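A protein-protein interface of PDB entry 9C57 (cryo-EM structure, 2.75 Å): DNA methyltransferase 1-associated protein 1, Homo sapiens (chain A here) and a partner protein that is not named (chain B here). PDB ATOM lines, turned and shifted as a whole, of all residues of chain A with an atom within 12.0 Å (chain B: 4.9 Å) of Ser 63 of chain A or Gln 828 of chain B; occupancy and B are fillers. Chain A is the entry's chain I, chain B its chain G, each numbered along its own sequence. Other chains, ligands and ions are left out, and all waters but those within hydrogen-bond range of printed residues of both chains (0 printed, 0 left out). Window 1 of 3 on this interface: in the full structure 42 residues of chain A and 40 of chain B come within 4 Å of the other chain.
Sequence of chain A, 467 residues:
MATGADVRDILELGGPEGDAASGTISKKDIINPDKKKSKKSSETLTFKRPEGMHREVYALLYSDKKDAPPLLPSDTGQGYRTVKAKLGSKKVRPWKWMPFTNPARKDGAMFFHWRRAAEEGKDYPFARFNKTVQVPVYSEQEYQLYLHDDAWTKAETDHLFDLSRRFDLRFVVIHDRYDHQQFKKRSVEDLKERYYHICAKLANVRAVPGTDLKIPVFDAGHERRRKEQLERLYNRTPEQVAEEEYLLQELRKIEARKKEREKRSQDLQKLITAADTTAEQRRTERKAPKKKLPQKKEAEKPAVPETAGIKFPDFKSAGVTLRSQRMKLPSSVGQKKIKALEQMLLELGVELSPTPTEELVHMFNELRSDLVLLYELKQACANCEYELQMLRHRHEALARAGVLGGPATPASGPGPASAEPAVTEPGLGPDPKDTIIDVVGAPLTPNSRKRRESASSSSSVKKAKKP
O of Ser 63 of chain A sits at hydrogen-bond distance from NE2 of Gln 828 of chain B, at 2.6 Å.
The guanidinium group (NH1) of Arg 831 of chain B lies within salt-bridge range of the side-chain carboxylate (OD2) of Asp 64 of chain A (3.7 Å).
The backbone carbonyl oxygen of Asp 67 of chain A sits at hydrogen-bond distance from the guanidinium group of Arg 831 of chain B (2.6 Å).
The backbone carbonyl oxygen (O) of Ala 68 of chain A is in hydrogen-bond range of the guanidinium group (NH2) of Arg 831 of chain B, at 2.4 Å.
The guanidinium group (NH1) of Arg 831 of chain B lies within hydrogen-bond range of the side-chain amide oxygen (OE1) of Gln 828 of chain B (2.9 Å).
NZ of Lys 65 of chain A lies within salt-bridge range of OD1 of Asp 67 of chain A, at 3.5 Å.
Asp 64 of chain A touches Gln 828 of chain B.
N of Pro 69 of chain A touches NH2 of Arg 831 of chain B, 3.7 Å away.
CB of Pro 69 of chain A touches CA of Trp 832 of chain B, at 3.9 Å.
Pro 70 of chain A touches Gln 828 of chain B (CG to O, 3.0 Å).
Pro 70 of chain A touches Arg 831 of chain B.
Pro 70 of chain A touches Trp 832 of chain B (O to CD1, 3.0 Å).
Trp 832 of chain B touches Leu 72 of chain A.
Of chain A, only Ser 63, Asp 64 and Pro 70 come within 4 Å of Gln 828 of chain B.
No residue of chain A comes within 4 Å of Thr 824 of chain B.
No residue of chain A comes within 4 Å of Asp 825 of chain B.
No residue of chain A comes within 4 Å of Glu 829 of chain B.
Printed residues of chain A within 4 Å of Arg 831 of chain B: Asp 64 (3.4 Å), Asp 67 (2.6 Å), Ala 68 (2.4 Å), Pro 69 (3.7 Å) and Pro 70 (3.9 Å).
Printed residues of chain B within 4 Å of Pro 70 of chain A: Gln 828, Arg 831 and Trp 832.
Of the printed residues of chain B, Leu 72 of chain A touches Trp 832.
The nearest residue of chain B that does not touch Ser 63 of chain A is Ala 827 of chain B (4.4 Å).
The nearest residue of chain A that does not touch Gln 828 of chain B is Ala 68 of chain A (5.2 Å).
Hydrophobic or aromatic side chains of chain B that line the printed part of chain A: Trp 832.
Hydrophobic or aromatic side chains of chain A that line the printed part of chain B: Pro 69, Pro 70 and Leu 72.
Among the printed residues, Asp or Glu carboxylates within 4 Å of a Lys or Arg side-chain nitrogen of the other chain: Asp 64 of chain A with Arg 831 of chain B (3.7 Å).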
ATOM      1  N   SER A  63     -20.735  -4.201  20.111  1.00  0.00           N
ATOM      2  CA  SER A  63     -21.878  -3.684  19.305  1.00  0.00           C
ATOM      3  C   SER A  63     -21.510  -2.395  18.587  1.00  0.00           C
ATOM      4  O   SER A  63     -21.258  -2.391  17.384  1.00  0.00           O
ATOM      5  CB  SER A  63     -23.099  -3.446  20.192  1.00  0.00           C
ATOM      6  OG  SER A  63     -23.629  -4.666  20.675  1.00  0.00           O
ATOM      7  N   ASP A  64     -21.478  -1.300  19.334  1.00  0.00           N
ATOM      8  CA  ASP A  64     -21.231   0.018  18.765  1.00  0.00           C
ATOM      9  C   ASP A  64     -20.937   0.977  19.911  1.00  0.00           C
ATOM     10  O   ASP A  64     -21.003   0.612  21.089  1.00  0.00           O
ATOM     11  CB  ASP A  64     -22.428   0.495  17.942  1.00  0.00           C
ATOM     12  CG  ASP A  64     -23.727   0.445  18.725  1.00  0.00           C
ATOM     13  OD1 ASP A  64     -23.841   1.159  19.743  1.00  0.00           O
ATOM     14  OD2 ASP A  64     -24.633  -0.314  18.329  1.00  0.00           O
ATOM     15  N   LYS A  65     -20.604   2.211  19.549  1.00  0.00           N
ATOM     16  CA  LYS A  65     -20.476   3.319  20.490  1.00  0.00           C
ATOM     17  C   LYS A  65     -21.119   4.575  19.906  1.00  0.00           C
ATOM     18  O   LYS A  65     -20.548   5.665  19.918  1.00  0.00           O
ATOM     19  CB  LYS A  65     -19.017   3.530  20.908  1.00  0.00           C
ATOM     20  CG  LYS A  65     -18.069   4.085  19.849  1.00  0.00           C
ATOM     21  CD  LYS A  65     -17.742   2.997  18.837  1.00  0.00           C
ATOM     22  CE  LYS A  65     -16.784   3.447  17.759  1.00  0.00           C
ATOM     23  NZ  LYS A  65     -16.936   2.583  16.552  1.00  0.00           N
ATOM     24  N   LYS A  66     -22.345   4.425  19.397  1.00  0.00           N
ATOM     25  CA  LYS A  66     -23.160   5.548  18.934  1.00  0.00           C
ATOM     26  C   LYS A  66     -22.446   6.307  17.809  1.00  0.00           C
ATOM     27  O   LYS A  66     -22.011   7.449  17.960  1.00  0.00           O
ATOM     28  CB  LYS A  66     -23.502   6.474  20.107  1.00  0.00           C
ATOM     29  CG  LYS A  66     -24.743   7.340  19.896  1.00  0.00           C
ATOM     30  CD  LYS A  66     -24.529   8.485  18.902  1.00  0.00           C
ATOM     31  CE  LYS A  66     -23.450   9.474  19.342  1.00  0.00           C
ATOM     32  NZ  LYS A  66     -23.034  10.379  18.233  1.00  0.00           N
ATOM     33  N   ASP A  67     -22.318   5.625  16.678  1.00  0.00           N
ATOM     34  CA  ASP A  67     -21.550   6.120  15.545  1.00  0.00           C
ATOM     35  C   ASP A  67     -22.402   6.100  14.278  1.00  0.00           C
ATOM     36  O   ASP A  67     -23.614   5.878  14.316  1.00  0.00           O
ATOM     37  CB  ASP A  67     -20.287   5.282  15.369  1.00  0.00           C
ATOM     38  CG  ASP A  67     -19.572   5.047  16.675  1.00  0.00           C
ATOM     39  OD1 ASP A  67     -19.950   4.093  17.381  1.00  0.00           O
ATOM     40  OD2 ASP A  67     -18.660   5.830  17.011  1.00  0.00           O
ATOM     41  N   ALA A  68     -21.744   6.327  13.142  1.00  0.00           N
ATOM     42  CA  ALA A  68     -22.427   6.342  11.864  1.00  0.00           C
ATOM     43  C   ALA A  68     -23.013   4.966  11.561  1.00  0.00           C
ATOM     44  O   ALA A  68     -22.504   3.946  12.032  1.00  0.00           O
ATOM     45  CB  ALA A  68     -21.462   6.762  10.759  1.00  0.00           C
ATOM     46  N   PRO A  69     -24.083   4.911  10.774  1.00  0.00           N
ATOM     47  CA  PRO A  69     -24.744   3.632  10.509  1.00  0.00           C
ATOM     48  C   PRO A  69     -23.856   2.724   9.679  1.00  0.00           C
ATOM     49  O   PRO A  69     -22.934   3.200   9.000  1.00  0.00           O
ATOM     50  CB  PRO A  69     -26.003   4.044   9.734  1.00  0.00           C
ATOM     51  CG  PRO A  69     -25.597   5.283   9.042  1.00  0.00           C
ATOM     52  CD  PRO A  69     -24.720   6.008  10.024  1.00  0.00           C
ATOM     53  N   PRO A  70     -24.093   1.414   9.707  1.00  0.00           N
ATOM     54  CA  PRO A  70     -23.290   0.507   8.885  1.00  0.00           C
ATOM     55  C   PRO A  70     -23.413   0.832   7.408  1.00  0.00           C
ATOM     56  O   PRO A  70     -24.353   1.489   6.958  1.00  0.00           O
ATOM     57  CB  PRO A  70     -23.875  -0.875   9.191  1.00  0.00           C
ATOM     58  CG  PRO A  70     -24.576  -0.729  10.454  1.00  0.00           C
ATOM     59  CD  PRO A  70     -25.047   0.683  10.556  1.00  0.00           C
ATOM     60  N   LEU A  71     -22.434   0.363   6.650  1.00  0.00           N
ATOM     61  CA  LEU A  71     -22.447   0.478   5.202  1.00  0.00           C
ATOM     62  C   LEU A  71     -22.727  -0.901   4.616  1.00  0.00           C
ATOM     63  O   LEU A  71     -22.071  -1.880   4.984  1.00  0.00           O
ATOM     64  CB  LEU A  71     -21.118   1.041   4.696  1.00  0.00           C
ATOM     65  CG  LEU A  71     -21.126   2.449   4.094  1.00  0.00           C
ATOM     66  CD1 LEU A  71     -21.572   3.477   5.089  1.00  0.00           C
ATOM     67  CD2 LEU A  71     -19.744   2.796   3.597  1.00  0.00           C
ATOM     68  N   LEU A  72     -23.710  -0.978   3.720  1.00  0.00           N
ATOM     69  CA  LEU A  72     -24.204  -2.245   3.201  1.00  0.00           C
ATOM     70  C   LEU A  72     -23.868  -2.405   1.721  1.00  0.00           C
ATOM     71  O   LEU A  72     -23.732  -1.411   1.002  1.00  0.00           O
ATOM     72  CB  LEU A  72     -25.724  -2.354   3.375  1.00  0.00           C
ATOM     73  CG  LEU A  72     -26.228  -3.078   4.621  1.00  0.00           C
ATOM     74  CD1 LEU A  72     -25.678  -2.433   5.879  1.00  0.00           C
ATOM     75  CD2 LEU A  72     -27.741  -3.087   4.645  1.00  0.00           C
ATOM     76  N   PRO A  73     -23.720  -3.637   1.238  1.00  0.00           N
ATOM     77  CA  PRO A  73     -23.580  -3.845  -0.206  1.00  0.00           C
ATOM     78  C   PRO A  73     -24.842  -3.453  -0.953  1.00  0.00           C
ATOM     79  O   PRO A  73     -25.962  -3.642  -0.473  1.00  0.00           O
ATOM     80  CB  PRO A  73     -23.316  -5.351  -0.330  1.00  0.00           C
ATOM     81  CG  PRO A  73     -22.857  -5.778   1.002  1.00  0.00           C
ATOM     82  CD  PRO A  73     -23.545  -4.891   1.987  1.00  0.00           C
ATOM     83  N   ALA B 823     -25.832 -10.871  17.395  1.00  0.00           N
ATOM     84  CA  ALA B 823     -26.250  -9.690  18.138  1.00  0.00           C
ATOM     85  C   ALA B 823     -25.604  -8.437  17.567  1.00  0.00           C
ATOM     86  O   ALA B 823     -26.254  -7.387  17.458  1.00  0.00           O
ATOM     87  CB  ALA B 823     -25.904  -9.848  19.616  1.00  0.00           C
ATOM     88  N   THR B 824     -24.326  -8.524  17.197  1.00  0.00           N
ATOM     89  CA  THR B 824     -23.707  -7.409  16.492  1.00  0.00           C
ATOM     90  C   THR B 824     -24.474  -7.097  15.215  1.00  0.00           C
ATOM     91  O   THR B 824     -24.740  -5.929  14.908  1.00  0.00           O
ATOM     92  CB  THR B 824     -22.246  -7.728  16.176  1.00  0.00           C
ATOM     93  OG1 THR B 824     -21.576  -8.155  17.369  1.00  0.00           O
ATOM     94  CG2 THR B 824     -21.538  -6.504  15.616  1.00  0.00           C
ATOM     95  N   ASP B 825     -24.856  -8.137  14.471  1.00  0.00           N
ATOM     96  CA  ASP B 825     -25.625  -7.934  13.247  1.00  0.00           C
ATOM     97  C   ASP B 825     -26.958  -7.255  13.536  1.00  0.00           C
ATOM     98  O   ASP B 825     -27.365  -6.342  12.817  1.00  0.00           O
ATOM     99  CB  ASP B 825     -25.856  -9.271  12.546  1.00  0.00           C
ATOM    100  CG  ASP B 825     -26.551  -9.111  11.213  1.00  0.00           C
ATOM    101  OD1 ASP B 825     -25.994  -8.424  10.333  1.00  0.00           O
ATOM    102  OD2 ASP B 825     -27.659  -9.664  11.048  1.00  0.00           O
ATOM    103  N   PHE B 826     -27.657  -7.699  14.579  1.00  0.00           N
ATOM    104  CA  PHE B 826     -28.948  -7.108  14.921  1.00  0.00           C
ATOM    105  C   PHE B 826     -28.807  -5.627  15.238  1.00  0.00           C
ATOM    106  O   PHE B 826     -29.546  -4.787  14.707  1.00  0.00           O
ATOM    107  CB  PHE B 826     -29.557  -7.835  16.116  1.00  0.00           C
ATOM    108  CG  PHE B 826     -30.581  -8.856  15.749  1.00  0.00           C
ATOM    109  CD1 PHE B 826     -30.240  -9.962  14.997  1.00  0.00           C
ATOM    110  CD2 PHE B 826     -31.889  -8.715  16.168  1.00  0.00           C
ATOM    111  CE1 PHE B 826     -31.184 -10.902  14.670  1.00  0.00           C
ATOM    112  CE2 PHE B 826     -32.835  -9.649  15.841  1.00  0.00           C
ATOM    113  CZ  PHE B 826     -32.484 -10.744  15.092  1.00  0.00           C
ATOM    114  N   ALA B 827     -27.871  -5.291  16.127  1.00  0.00           N
ATOM    115  CA  ALA B 827     -27.700  -3.896  16.510  1.00  0.00           C
ATOM    116  C   ALA B 827     -27.313  -3.045  15.310  1.00  0.00           C
ATOM    117  O   ALA B 827     -27.872  -1.959  15.099  1.00  0.00           O
ATOM    118  CB  ALA B 827     -26.648  -3.781  17.612  1.00  0.00           C
ATOM    119  N   GLN B 828     -26.372  -3.528  14.499  1.00  0.00           N
ATOM    120  CA  GLN B 828     -25.924  -2.744  13.358  1.00  0.00           C
ATOM    121  C   GLN B 828     -27.028  -2.603  12.318  1.00  0.00           C
ATOM    122  O   GLN B 828     -27.155  -1.554  11.683  1.00  0.00           O
ATOM    123  CB  GLN B 828     -24.678  -3.383  12.751  1.00  0.00           C
ATOM    124  CG  GLN B 828     -23.479  -3.351  13.678  1.00  0.00           C
ATOM    125  CD  GLN B 828     -23.045  -1.945  14.023  1.00  0.00           C
ATOM    126  OE1 GLN B 828     -23.542  -0.974  13.460  1.00  0.00           O
ATOM    127  NE2 GLN B 828     -22.110  -1.830  14.956  1.00  0.00           N
ATOM    128  N   GLU B 829     -27.842  -3.640  12.135  1.00  0.00           N
ATOM    129  CA  GLU B 829     -28.953  -3.543  11.199  1.00  0.00           C
ATOM    130  C   GLU B 829     -29.983  -2.532  11.676  1.00  0.00           C
ATOM    131  O   GLU B 829     -30.521  -1.763  10.874  1.00  0.00           O
ATOM    132  CB  GLU B 829     -29.597  -4.912  11.006  1.00  0.00           C
ATOM    133  CG  GLU B 829     -30.757  -4.902  10.043  1.00  0.00           C
ATOM    134  CD  GLU B 829     -31.067  -6.272   9.500  1.00  0.00           C
ATOM    135  OE1 GLU B 829     -31.865  -6.994  10.131  1.00  0.00           O
ATOM    136  OE2 GLU B 829     -30.509  -6.631   8.444  1.00  0.00           O
ATOM    137  N   ARG B 830     -30.277  -2.519  12.976  1.00  0.00           N
ATOM    138  CA  ARG B 830     -31.190  -1.509  13.500  1.00  0.00           C
ATOM    139  C   ARG B 830     -30.630  -0.113  13.277  1.00  0.00           C
ATOM    140  O   ARG B 830     -31.367   0.813  12.916  1.00  0.00           O
ATOM    141  CB  ARG B 830     -31.448  -1.751  14.986  1.00  0.00           C
ATOM    142  CG  ARG B 830     -32.466  -0.810  15.607  1.00  0.00           C
ATOM    143  CD  ARG B 830     -32.188  -0.616  17.079  1.00  0.00           C
ATOM    144  NE  ARG B 830     -31.864  -1.877  17.731  1.00  0.00           N
ATOM    145  CZ  ARG B 830     -32.750  -2.818  18.017  1.00  0.00           C
ATOM    146  NH1 ARG B 830     -34.031  -2.673  17.724  1.00  0.00           N
ATOM    147  NH2 ARG B 830     -32.340  -3.937  18.605  1.00  0.00           N
ATOM    148  N   ARG B 831     -29.325   0.058  13.489  1.00  0.00           N
ATOM    149  CA  ARG B 831     -28.700   1.355  13.254  1.00  0.00           C
ATOM    150  C   ARG B 831     -28.805   1.761  11.786  1.00  0.00           C
ATOM    151  O   ARG B 831     -29.156   2.905  11.465  1.00  0.00           O
ATOM    152  CB  ARG B 831     -27.243   1.303  13.702  1.00  0.00           C
ATOM    153  CG  ARG B 831     -27.076   1.054  15.201  1.00  0.00           C
ATOM    154  CD  ARG B 831     -26.614   2.292  15.961  1.00  0.00           C
ATOM    155  NE  ARG B 831     -25.610   3.056  15.232  1.00  0.00           N
ATOM    156  CZ  ARG B 831     -24.448   2.571  14.814  1.00  0.00           C
ATOM    157  NH1 ARG B 831     -24.059   1.344  15.117  1.00  0.00           N
ATOM    158  NH2 ARG B 831     -23.655   3.338  14.075  1.00  0.00           N
ATOM    159  N   TRP B 832     -28.511   0.832  10.877  1.00  0.00           N
ATOM    160  CA  TRP B 832     -28.620   1.140   9.457  1.00  0.00           C
ATOM    161  C   TRP B 832     -30.047   1.500   9.088  1.00  0.00           C
ATOM    162  O   TRP B 832     -30.274   2.424   8.307  1.00  0.00           O
ATOM    163  CB  TRP B 832     -28.158  -0.033   8.597  1.00  0.00           C
ATOM    164  CG  TRP B 832     -28.194   0.296   7.131  1.00  0.00           C
ATOM    165  CD1 TRP B 832     -27.228   0.931   6.416  1.00  0.00           C
ATOM    166  CD2 TRP B 832     -29.258   0.024   6.211  1.00  0.00           C
ATOM    167  NE1 TRP B 832     -27.614   1.066   5.107  1.00  0.00           N
ATOM    168  CE2 TRP B 832     -28.860   0.518   4.956  1.00  0.00           C
ATOM    169  CE3 TRP B 832     -30.507  -0.591   6.327  1.00  0.00           C
ATOM    170  CZ2 TRP B 832     -29.663   0.415   3.825  1.00  0.00           C
ATOM    171  CZ3 TRP B 832     -31.303  -0.691   5.201  1.00  0.00           C
ATOM    172  CH2 TRP B 832     -30.878  -0.192   3.969  1.00  0.00           C
